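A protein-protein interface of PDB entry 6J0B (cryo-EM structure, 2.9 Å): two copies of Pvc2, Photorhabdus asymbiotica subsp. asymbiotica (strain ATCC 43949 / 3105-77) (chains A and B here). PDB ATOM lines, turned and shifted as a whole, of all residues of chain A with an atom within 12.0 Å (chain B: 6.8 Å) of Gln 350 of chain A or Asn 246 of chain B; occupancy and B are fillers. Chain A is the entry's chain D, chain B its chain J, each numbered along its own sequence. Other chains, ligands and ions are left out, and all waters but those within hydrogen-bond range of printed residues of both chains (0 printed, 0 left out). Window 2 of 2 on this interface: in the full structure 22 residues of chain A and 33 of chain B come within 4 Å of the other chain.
The backbone carbonyl oxygen (O) of Gln 350 of chain A lies close to the backbone carbonyl oxygen (O) of Leu 335 of chain B (2.7 Å). The backbone carbonyl oxygen of Gln 347 of chain A lies within hydrogen-bond range of the backbone NH of Val 333 of chain B (2.7 Å). The backbone carbonyl oxygen of Thr 349 of chain A sits at hydrogen-bond distance from the backbone NH of Leu 335 of chain B (3.3 Å). The backbone NH (N) of Thr 349 of chain A lies within hydrogen-bond range of the backbone carbonyl oxygen (O) of Val 333 of chain B (2.6 Å).
Val 333 of chain B touches Phe 348 of chain A. Thr 349 of chain A touches Gly 334 of chain B. Asn 246 of chain B touches Gln 350 of chain A (OD1 to CG, 3.2 Å). CZ3 of Trp 247 of chain B touches NE2 of Gln 350 of chain A, at 3.3 Å. CG1 of Val 252 of chain B touches NE2 of Gln 350 of chain A, 3.9 Å away. Gln 350 of chain A touches Phe 256 of chain B. Gly 334 of chain B touches Val 352 of chain A. Val 352 of chain A touches Leu 335 of chain B. Val 352 of chain A touches Ala 336 of chain B (CG2 to N, 3.9 Å).
Asn 246 of chain B touches just one residue of chain A: Gln 350. No residue of chain A comes within 4 Å of Asp 245 of chain B. Of chain A, only Gln 350 (3.3 Å) comes within 4 Å of Trp 247 of chain B. No residue of chain A comes within 4 Å of Arg 248 of chain B. Of chain A, only Thr 349 and Val 352 come within 4 Å of Gly 334 of chain B. Ala 336 of chain B touches just one residue of chain A: Val 352. Of the printed residues of chain A, Val 333 of chain B touches Gln 347 (2.7 Å), Phe 348 (3.2 Å) and Thr 349 (2.6 Å). Of the printed residues of chain B, Thr 349 of chain A touches Val 333 (2.6 Å), Gly 334 (3.2 Å) and Leu 335 (3.3 Å). Printed residues of chain B within 4 Å of Phe 348 of chain A: Val 333. Arg 253 of chain B touches none of the printed residues of chain A. The nearest residue of chain A that does not touch Asn 246 of chain B is Asp 351 of chain A (6.0 Å). The nearest printed residue of chain B that does not touch Thr 349 of chain A is Phe 256 of chain B (4.1 Å).
Hydrophobic or aromatic side chains of chain B that line the printed part of chain A: Trp 247, Val 252, Phe 256 and Val 333. Hydrophobic or aromatic side chains of chain A within 4 Å of the printed part of chain B: Phe 348 and Val 352. Among the printed residues, 13 pairs touch across the chains. Among the printed residues, no Asp or Glu carboxylate lies within 4 Å of a Lys or Arg side-chain nitrogen of the other chain.
No position is printed for both chains. Of the 13 pairs that touch across the chains among the printed residues, none has its exchanged pair printed and touching as well.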
ATOM      1  N   LEU A 346      12.015  -2.921 -11.035  1.00  0.00           N
ATOM      2  CA  LEU A 346      12.071  -4.093 -10.175  1.00  0.00           C
ATOM      3  C   LEU A 346      13.286  -4.914 -10.545  1.00  0.00           C
ATOM      4  O   LEU A 346      13.499  -5.199 -11.724  1.00  0.00           O
ATOM      5  CB  LEU A 346      10.836  -4.959 -10.352  1.00  0.00           C
ATOM      6  CG  LEU A 346       9.573  -4.537  -9.669  1.00  0.00           C
ATOM      7  CD1 LEU A 346       8.424  -5.191 -10.396  1.00  0.00           C
ATOM      8  CD2 LEU A 346       9.685  -5.041  -8.266  1.00  0.00           C
ATOM      9  N   GLN A 347      14.061  -5.313  -9.548  1.00  0.00           N
ATOM     10  CA  GLN A 347      15.126  -6.280  -9.743  1.00  0.00           C
ATOM     11  C   GLN A 347      14.777  -7.548  -8.986  1.00  0.00           C
ATOM     12  O   GLN A 347      14.631  -7.524  -7.761  1.00  0.00           O
ATOM     13  CB  GLN A 347      16.468  -5.722  -9.293  1.00  0.00           C
ATOM     14  CG  GLN A 347      17.043  -4.757 -10.287  1.00  0.00           C
ATOM     15  CD  GLN A 347      17.497  -3.495  -9.632  1.00  0.00           C
ATOM     16  OE1 GLN A 347      17.522  -3.405  -8.411  1.00  0.00           O
ATOM     17  NE2 GLN A 347      17.861  -2.504 -10.434  1.00  0.00           N
ATOM     18  N   PHE A 348      14.626  -8.645  -9.716  1.00  0.00           N
ATOM     19  CA  PHE A 348      14.271  -9.929  -9.136  1.00  0.00           C
ATOM     20  C   PHE A 348      15.512 -10.803  -9.074  1.00  0.00           C
ATOM     21  O   PHE A 348      16.130 -11.087 -10.104  1.00  0.00           O
ATOM     22  CB  PHE A 348      13.157 -10.604  -9.930  1.00  0.00           C
ATOM     23  CG  PHE A 348      11.797 -10.110  -9.572  1.00  0.00           C
ATOM     24  CD1 PHE A 348      11.320  -8.930 -10.102  1.00  0.00           C
ATOM     25  CD2 PHE A 348      11.005 -10.809  -8.683  1.00  0.00           C
ATOM     26  CE1 PHE A 348      10.073  -8.463  -9.764  1.00  0.00           C
ATOM     27  CE2 PHE A 348       9.755 -10.345  -8.346  1.00  0.00           C
ATOM     28  CZ  PHE A 348       9.293  -9.170  -8.894  1.00  0.00           C
ATOM     29  N   THR A 349      15.872 -11.213  -7.865  1.00  0.00           N
ATOM     30  CA  THR A 349      17.049 -12.028  -7.618  1.00  0.00           C
ATOM     31  C   THR A 349      16.607 -13.454  -7.322  1.00  0.00           C
ATOM     32  O   THR A 349      15.611 -13.672  -6.631  1.00  0.00           O
ATOM     33  CB  THR A 349      17.862 -11.467  -6.449  1.00  0.00           C
ATOM     34  OG1 THR A 349      17.842 -10.035  -6.495  1.00  0.00           O
ATOM     35  CG2 THR A 349      19.293 -11.919  -6.541  1.00  0.00           C
ATOM     36  N   GLN A 350      17.343 -14.425  -7.857  1.00  0.00           N
ATOM     37  CA  GLN A 350      16.919 -15.813  -7.720  1.00  0.00           C
ATOM     38  C   GLN A 350      17.316 -16.389  -6.365  1.00  0.00           C
ATOM     39  O   GLN A 350      16.622 -17.257  -5.828  1.00  0.00           O
ATOM     40  CB  GLN A 350      17.489 -16.639  -8.874  1.00  0.00           C
ATOM     41  CG  GLN A 350      17.227 -18.136  -8.810  1.00  0.00           C
ATOM     42  CD  GLN A 350      15.780 -18.518  -8.958  1.00  0.00           C
ATOM     43  OE1 GLN A 350      15.033 -18.547  -7.984  1.00  0.00           O
ATOM     44  NE2 GLN A 350      15.380 -18.848 -10.175  1.00  0.00           N
ATOM     45  N   ASP A 351      18.409 -15.919  -5.780  1.00  0.00           N
ATOM     46  CA  ASP A 351      18.811 -16.392  -4.463  1.00  0.00           C
ATOM     47  C   ASP A 351      18.462 -15.362  -3.397  1.00  0.00           C
ATOM     48  O   ASP A 351      18.681 -14.161  -3.578  1.00  0.00           O
ATOM     49  CB  ASP A 351      20.306 -16.729  -4.417  1.00  0.00           C
ATOM     50  CG  ASP A 351      21.185 -15.587  -4.870  1.00  0.00           C
ATOM     51  OD1 ASP A 351      20.698 -14.715  -5.611  1.00  0.00           O
ATOM     52  OD2 ASP A 351      22.375 -15.571  -4.497  1.00  0.00           O
ATOM     53  N   VAL A 352      17.905 -15.843  -2.291  1.00  0.00           N
ATOM     54  CA  VAL A 352      17.470 -14.999  -1.185  1.00  0.00           C
ATOM     55  C   VAL A 352      18.615 -14.891  -0.195  1.00  0.00           C
ATOM     56  O   VAL A 352      19.048 -15.895   0.381  1.00  0.00           O
ATOM     57  CB  VAL A 352      16.216 -15.555  -0.503  1.00  0.00           C
ATOM     58  CG1 VAL A 352      15.910 -14.767   0.747  1.00  0.00           C
ATOM     59  CG2 VAL A 352      15.074 -15.459  -1.420  1.00  0.00           C
ATOM     60  N   GLU A 353      19.092 -13.674   0.018  1.00  0.00           N
ATOM     61  CA  GLU A 353      20.137 -13.428   0.995  1.00  0.00           C
ATOM     62  C   GLU A 353      20.065 -12.000   1.524  1.00  0.00           C
ATOM     63  O   GLU A 353      20.478 -11.058   0.849  1.00  0.00           O
ATOM     64  CB  GLU A 353      21.515 -13.698   0.388  1.00  0.00           C
ATOM     65  CG  GLU A 353      22.213 -14.908   0.978  1.00  0.00           C
ATOM     66  CD  GLU A 353      22.557 -14.721   2.442  1.00  0.00           C
ATOM     67  OE1 GLU A 353      22.855 -13.576   2.848  1.00  0.00           O
ATOM     68  OE2 GLU A 353      22.527 -15.719   3.189  1.00  0.00           O
ATOM     69  N   GLU B 242      16.648 -24.195 -21.295  1.00  0.00           N
ATOM     70  CA  GLU B 242      17.892 -23.763 -20.674  1.00  0.00           C
ATOM     71  C   GLU B 242      18.444 -24.856 -19.772  1.00  0.00           C
ATOM     72  O   GLU B 242      17.733 -25.405 -18.927  1.00  0.00           O
ATOM     73  CB  GLU B 242      17.668 -22.496 -19.857  1.00  0.00           C
ATOM     74  CG  GLU B 242      18.925 -21.920 -19.239  1.00  0.00           C
ATOM     75  CD  GLU B 242      19.599 -20.900 -20.133  1.00  0.00           C
ATOM     76  OE1 GLU B 242      19.042 -19.795 -20.301  1.00  0.00           O
ATOM     77  OE2 GLU B 242      20.684 -21.202 -20.672  1.00  0.00           O
ATOM     78  N   ASP B 243      19.725 -25.165 -19.944  1.00  0.00           N
ATOM     79  CA  ASP B 243      20.370 -26.195 -19.144  1.00  0.00           C
ATOM     80  C   ASP B 243      20.975 -25.656 -17.854  1.00  0.00           C
ATOM     81  O   ASP B 243      21.384 -26.454 -17.004  1.00  0.00           O
ATOM     82  CB  ASP B 243      21.453 -26.898 -19.966  1.00  0.00           C
ATOM     83  CG  ASP B 243      21.824 -28.257 -19.404  1.00  0.00           C
ATOM     84  OD1 ASP B 243      22.959 -28.716 -19.646  1.00  0.00           O
ATOM     85  OD2 ASP B 243      20.988 -28.849 -18.689  1.00  0.00           O
ATOM     86  N   LYS B 244      21.037 -24.333 -17.691  1.00  0.00           N
ATOM     87  CA  LYS B 244      21.608 -23.740 -16.491  1.00  0.00           C
ATOM     88  C   LYS B 244      20.771 -24.087 -15.267  1.00  0.00           C
ATOM     89  O   LYS B 244      19.557 -24.287 -15.353  1.00  0.00           O
ATOM     90  CB  LYS B 244      21.704 -22.221 -16.634  1.00  0.00           C
ATOM     91  CG  LYS B 244      22.589 -21.730 -17.767  1.00  0.00           C
ATOM     92  CD  LYS B 244      22.841 -20.235 -17.620  1.00  0.00           C
ATOM     93  CE  LYS B 244      23.657 -19.669 -18.769  1.00  0.00           C
ATOM     94  NZ  LYS B 244      22.848 -19.487 -20.005  1.00  0.00           N
ATOM     95  N   ASP B 245      21.438 -24.159 -14.115  1.00  0.00           N
ATOM     96  CA  ASP B 245      20.794 -24.634 -12.895  1.00  0.00           C
ATOM     97  C   ASP B 245      19.814 -23.627 -12.311  1.00  0.00           C
ATOM     98  O   ASP B 245      19.052 -23.979 -11.406  1.00  0.00           O
ATOM     99  CB  ASP B 245      21.854 -24.996 -11.856  1.00  0.00           C
ATOM    100  CG  ASP B 245      23.011 -24.012 -11.835  1.00  0.00           C
ATOM    101  OD1 ASP B 245      22.994 -23.049 -12.632  1.00  0.00           O
ATOM    102  OD2 ASP B 245      23.940 -24.203 -11.022  1.00  0.00           O
ATOM    103  N   ASN B 246      19.811 -22.392 -12.808  1.00  0.00           N
ATOM    104  CA  ASN B 246      18.877 -21.387 -12.322  1.00  0.00           C
ATOM    105  C   ASN B 246      17.476 -21.604 -12.870  1.00  0.00           C
ATOM    106  O   ASN B 246      16.501 -21.610 -12.111  1.00  0.00           O
ATOM    107  CB  ASN B 246      19.368 -19.996 -12.706  1.00  0.00           C
ATOM    108  CG  ASN B 246      19.350 -19.051 -11.551  1.00  0.00           C
ATOM    109  OD1 ASN B 246      19.597 -19.456 -10.423  1.00  0.00           O
ATOM    110  ND2 ASN B 246      19.057 -17.784 -11.813  1.00  0.00           N
ATOM    111  N   TRP B 247      17.358 -21.784 -14.183  1.00  0.00           N
ATOM    112  CA  TRP B 247      16.063 -21.848 -14.843  1.00  0.00           C
ATOM    113  C   TRP B 247      15.866 -23.186 -15.534  1.00  0.00           C
ATOM    114  O   TRP B 247      15.456 -23.233 -16.697  1.00  0.00           O
ATOM    115  CB  TRP B 247      15.923 -20.716 -15.858  1.00  0.00           C
ATOM    116  CG  TRP B 247      16.112 -19.361 -15.274  1.00  0.00           C
ATOM    117  CD1 TRP B 247      17.126 -18.492 -15.533  1.00  0.00           C
ATOM    118  CD2 TRP B 247      15.264 -18.717 -14.320  1.00  0.00           C
ATOM    119  NE1 TRP B 247      16.962 -17.344 -14.802  1.00  0.00           N
ATOM    120  CE2 TRP B 247      15.824 -17.459 -14.049  1.00  0.00           C
ATOM    121  CE3 TRP B 247      14.084 -19.083 -13.670  1.00  0.00           C
ATOM    122  CZ2 TRP B 247      15.246 -16.567 -13.157  1.00  0.00           C
ATOM    123  CZ3 TRP B 247      13.515 -18.200 -12.788  1.00  0.00           C
ATOM    124  CH2 TRP B 247      14.094 -16.956 -12.538  1.00  0.00           C
ATOM    125  N   ARG B 248      16.164 -24.275 -14.833  1.00  0.00           N
ATOM    126  CA  ARG B 248      16.111 -25.587 -15.460  1.00  0.00           C
ATOM    127  C   ARG B 248      14.681 -26.078 -15.635  1.00  0.00           C
ATOM    128  O   ARG B 248      14.371 -26.724 -16.638  1.00  0.00           O
ATOM    129  CB  ARG B 248      16.916 -26.589 -14.640  1.00  0.00           C
ATOM    130  CG  ARG B 248      17.171 -27.890 -15.353  1.00  0.00           C
ATOM    131  CD  ARG B 248      17.720 -28.933 -14.411  1.00  0.00           C
ATOM    132  NE  ARG B 248      18.870 -28.456 -13.656  1.00  0.00           N
ATOM    133  CZ  ARG B 248      20.116 -28.459 -14.110  1.00  0.00           C
ATOM    134  NH1 ARG B 248      21.100 -28.010 -13.345  1.00  0.00           N
ATOM    135  NH2 ARG B 248      20.384 -28.906 -15.328  1.00  0.00           N
ATOM    136  N   TYR B 249      13.797 -25.773 -14.692  1.00  0.00           N
ATOM    137  CA  TYR B 249      12.465 -26.359 -14.647  1.00  0.00           C
ATOM    138  C   TYR B 249      11.397 -25.333 -15.001  1.00  0.00           C
ATOM    139  O   TYR B 249      11.511 -24.161 -14.632  1.00  0.00           O
ATOM    140  CB  TYR B 249      12.185 -26.940 -13.262  1.00  0.00           C
ATOM    141  CG  TYR B 249      13.154 -28.015 -12.849  1.00  0.00           C
ATOM    142  CD1 TYR B 249      13.036 -29.304 -13.342  1.00  0.00           C
ATOM    143  CD2 TYR B 249      14.185 -27.742 -11.962  1.00  0.00           C
ATOM    144  CE1 TYR B 249      13.917 -30.288 -12.971  1.00  0.00           C
ATOM    145  CE2 TYR B 249      15.072 -28.722 -11.584  1.00  0.00           C
ATOM    146  CZ  TYR B 249      14.933 -29.994 -12.091  1.00  0.00           C
ATOM    147  OH  TYR B 249      15.815 -30.977 -11.714  1.00  0.00           O
ATOM    148  N   VAL B 252       9.682 -23.381 -11.983  1.00  0.00           N
ATOM    149  CA  VAL B 252      10.428 -22.262 -11.419  1.00  0.00           C
ATOM    150  C   VAL B 252      10.357 -21.053 -12.340  1.00  0.00           C
ATOM    151  O   VAL B 252      10.247 -19.912 -11.879  1.00  0.00           O
ATOM    152  CB  VAL B 252      11.880 -22.688 -11.141  1.00  0.00           C
ATOM    153  CG1 VAL B 252      12.647 -21.585 -10.441  1.00  0.00           C
ATOM    154  CG2 VAL B 252      11.898 -23.948 -10.304  1.00  0.00           C
ATOM    155  N   ARG B 253      10.398 -21.281 -13.653  1.00  0.00           N
ATOM    156  CA  ARG B 253      10.317 -20.177 -14.603  1.00  0.00           C
ATOM    157  C   ARG B 253       8.915 -19.586 -14.647  1.00  0.00           C
ATOM    158  O   ARG B 253       8.756 -18.365 -14.738  1.00  0.00           O
ATOM    159  CB  ARG B 253      10.749 -20.653 -15.988  1.00  0.00           C
ATOM    160  CG  ARG B 253      10.685 -19.607 -17.088  1.00  0.00           C
ATOM    161  CD  ARG B 253      11.739 -18.529 -16.924  1.00  0.00           C
ATOM    162  NE  ARG B 253      11.217 -17.348 -16.246  1.00  0.00           N
ATOM    163  CZ  ARG B 253      11.921 -16.247 -16.018  1.00  0.00           C
ATOM    164  NH1 ARG B 253      13.181 -16.171 -16.415  1.00  0.00           N
ATOM    165  NH2 ARG B 253      11.365 -15.222 -15.393  1.00  0.00           N
ATOM    166  N   PHE B 256       8.239 -17.403 -11.410  1.00  0.00           N
ATOM    167  CA  PHE B 256       8.822 -16.070 -11.493  1.00  0.00           C
ATOM    168  C   PHE B 256       8.103 -15.193 -12.504  1.00  0.00           C
ATOM    169  O   PHE B 256       8.033 -13.978 -12.313  1.00  0.00           O
ATOM    170  CB  PHE B 256      10.302 -16.166 -11.841  1.00  0.00           C
ATOM    171  CG  PHE B 256      11.191 -16.231 -10.646  1.00  0.00           C
ATOM    172  CD1 PHE B 256      11.922 -15.124 -10.253  1.00  0.00           C
ATOM    173  CD2 PHE B 256      11.283 -17.392  -9.900  1.00  0.00           C
ATOM    174  CE1 PHE B 256      12.737 -15.179  -9.149  1.00  0.00           C
ATOM    175  CE2 PHE B 256      12.097 -17.453  -8.793  1.00  0.00           C
ATOM    176  CZ  PHE B 256      12.824 -16.345  -8.417  1.00  0.00           C
ATOM    177  N   VAL B 333      13.807  -7.638  -5.157  1.00  0.00           N
ATOM    178  CA  VAL B 333      13.000  -8.747  -4.670  1.00  0.00           C
ATOM    179  C   VAL B 333      13.783 -10.031  -4.905  1.00  0.00           C
ATOM    180  O   VAL B 333      14.364 -10.217  -5.978  1.00  0.00           O
ATOM    181  CB  VAL B 333      11.631  -8.797  -5.374  1.00  0.00           C
ATOM    182  CG1 VAL B 333      10.768  -9.885  -4.800  1.00  0.00           C
ATOM    183  CG2 VAL B 333      10.916  -7.465  -5.268  1.00  0.00           C
ATOM    184  N   GLY B 334      13.824 -10.898  -3.904  1.00  0.00           N
ATOM    185  CA  GLY B 334      14.379 -12.225  -4.074  1.00  0.00           C
ATOM    186  C   GLY B 334      13.363 -13.267  -3.661  1.00  0.00           C
ATOM    187  O   GLY B 334      12.526 -13.028  -2.799  1.00  0.00           O
ATOM    188  N   LEU B 335      13.428 -14.424  -4.312  1.00  0.00           N
ATOM    189  CA  LEU B 335      12.504 -15.519  -4.044  1.00  0.00           C
ATOM    190  C   LEU B 335      13.280 -16.821  -3.929  1.00  0.00           C
ATOM    191  O   LEU B 335      14.422 -16.918  -4.366  1.00  0.00           O
ATOM    192  CB  LEU B 335      11.450 -15.670  -5.140  1.00  0.00           C
ATOM    193  CG  LEU B 335      10.660 -14.461  -5.616  1.00  0.00           C
ATOM    194  CD1 LEU B 335       9.766 -14.888  -6.751  1.00  0.00           C
ATOM    195  CD2 LEU B 335       9.845 -13.900  -4.489  1.00  0.00           C
ATOM    196  N   ALA B 336      12.659 -17.820  -3.314  1.00  0.00           N
ATOM    197  CA  ALA B 336      13.258 -19.146  -3.184  1.00  0.00           C
ATOM    198  C   ALA B 336      12.204 -20.169  -3.590  1.00  0.00           C
ATOM    199  O   ALA B 336      11.370 -20.565  -2.773  1.00  0.00           O
ATOM    200  CB  ALA B 336      13.759 -19.392  -1.768  1.00  0.00           C
ATOM    201  N   ALA B 337      12.246 -20.597  -4.846  1.00  0.00           N
ATOM    202  CA  ALA B 337      11.265 -21.538  -5.354  1.00  0.00           C
ATOM    203  C   ALA B 337      11.598 -22.959  -4.909  1.00  0.00           C
ATOM    204  O   ALA B 337      12.699 -23.254  -4.439  1.00  0.00           O
ATOM    205  CB  ALA B 337      11.192 -21.460  -6.875  1.00  0.00           C
ATOM    206  N   ARG B 339      12.070 -26.923  -5.901  1.00  0.00           N
ATOM    207  CA  ARG B 339      12.391 -27.699  -7.087  1.00  0.00           C
ATOM    208  C   ARG B 339      11.673 -29.043  -7.041  1.00  0.00           C
ATOM    209  O   ARG B 339      11.457 -29.600  -5.962  1.00  0.00           O
ATOM    210  CB  ARG B 339      13.897 -27.925  -7.189  1.00  0.00           C
ATOM    211  CG  ARG B 339      14.735 -26.680  -6.978  1.00  0.00           C
ATOM    212  CD  ARG B 339      14.356 -25.581  -7.944  1.00  0.00           C
ATOM    213  NE  ARG B 339      14.984 -24.314  -7.594  1.00  0.00           N
ATOM    214  CZ  ARG B 339      16.025 -23.801  -8.236  1.00  0.00           C
ATOM    215  NH1 ARG B 339      16.538 -22.642  -7.850  1.00  0.00           N
ATOM    216  NH2 ARG B 339      16.547 -24.441  -9.270  1.00  0.00           N
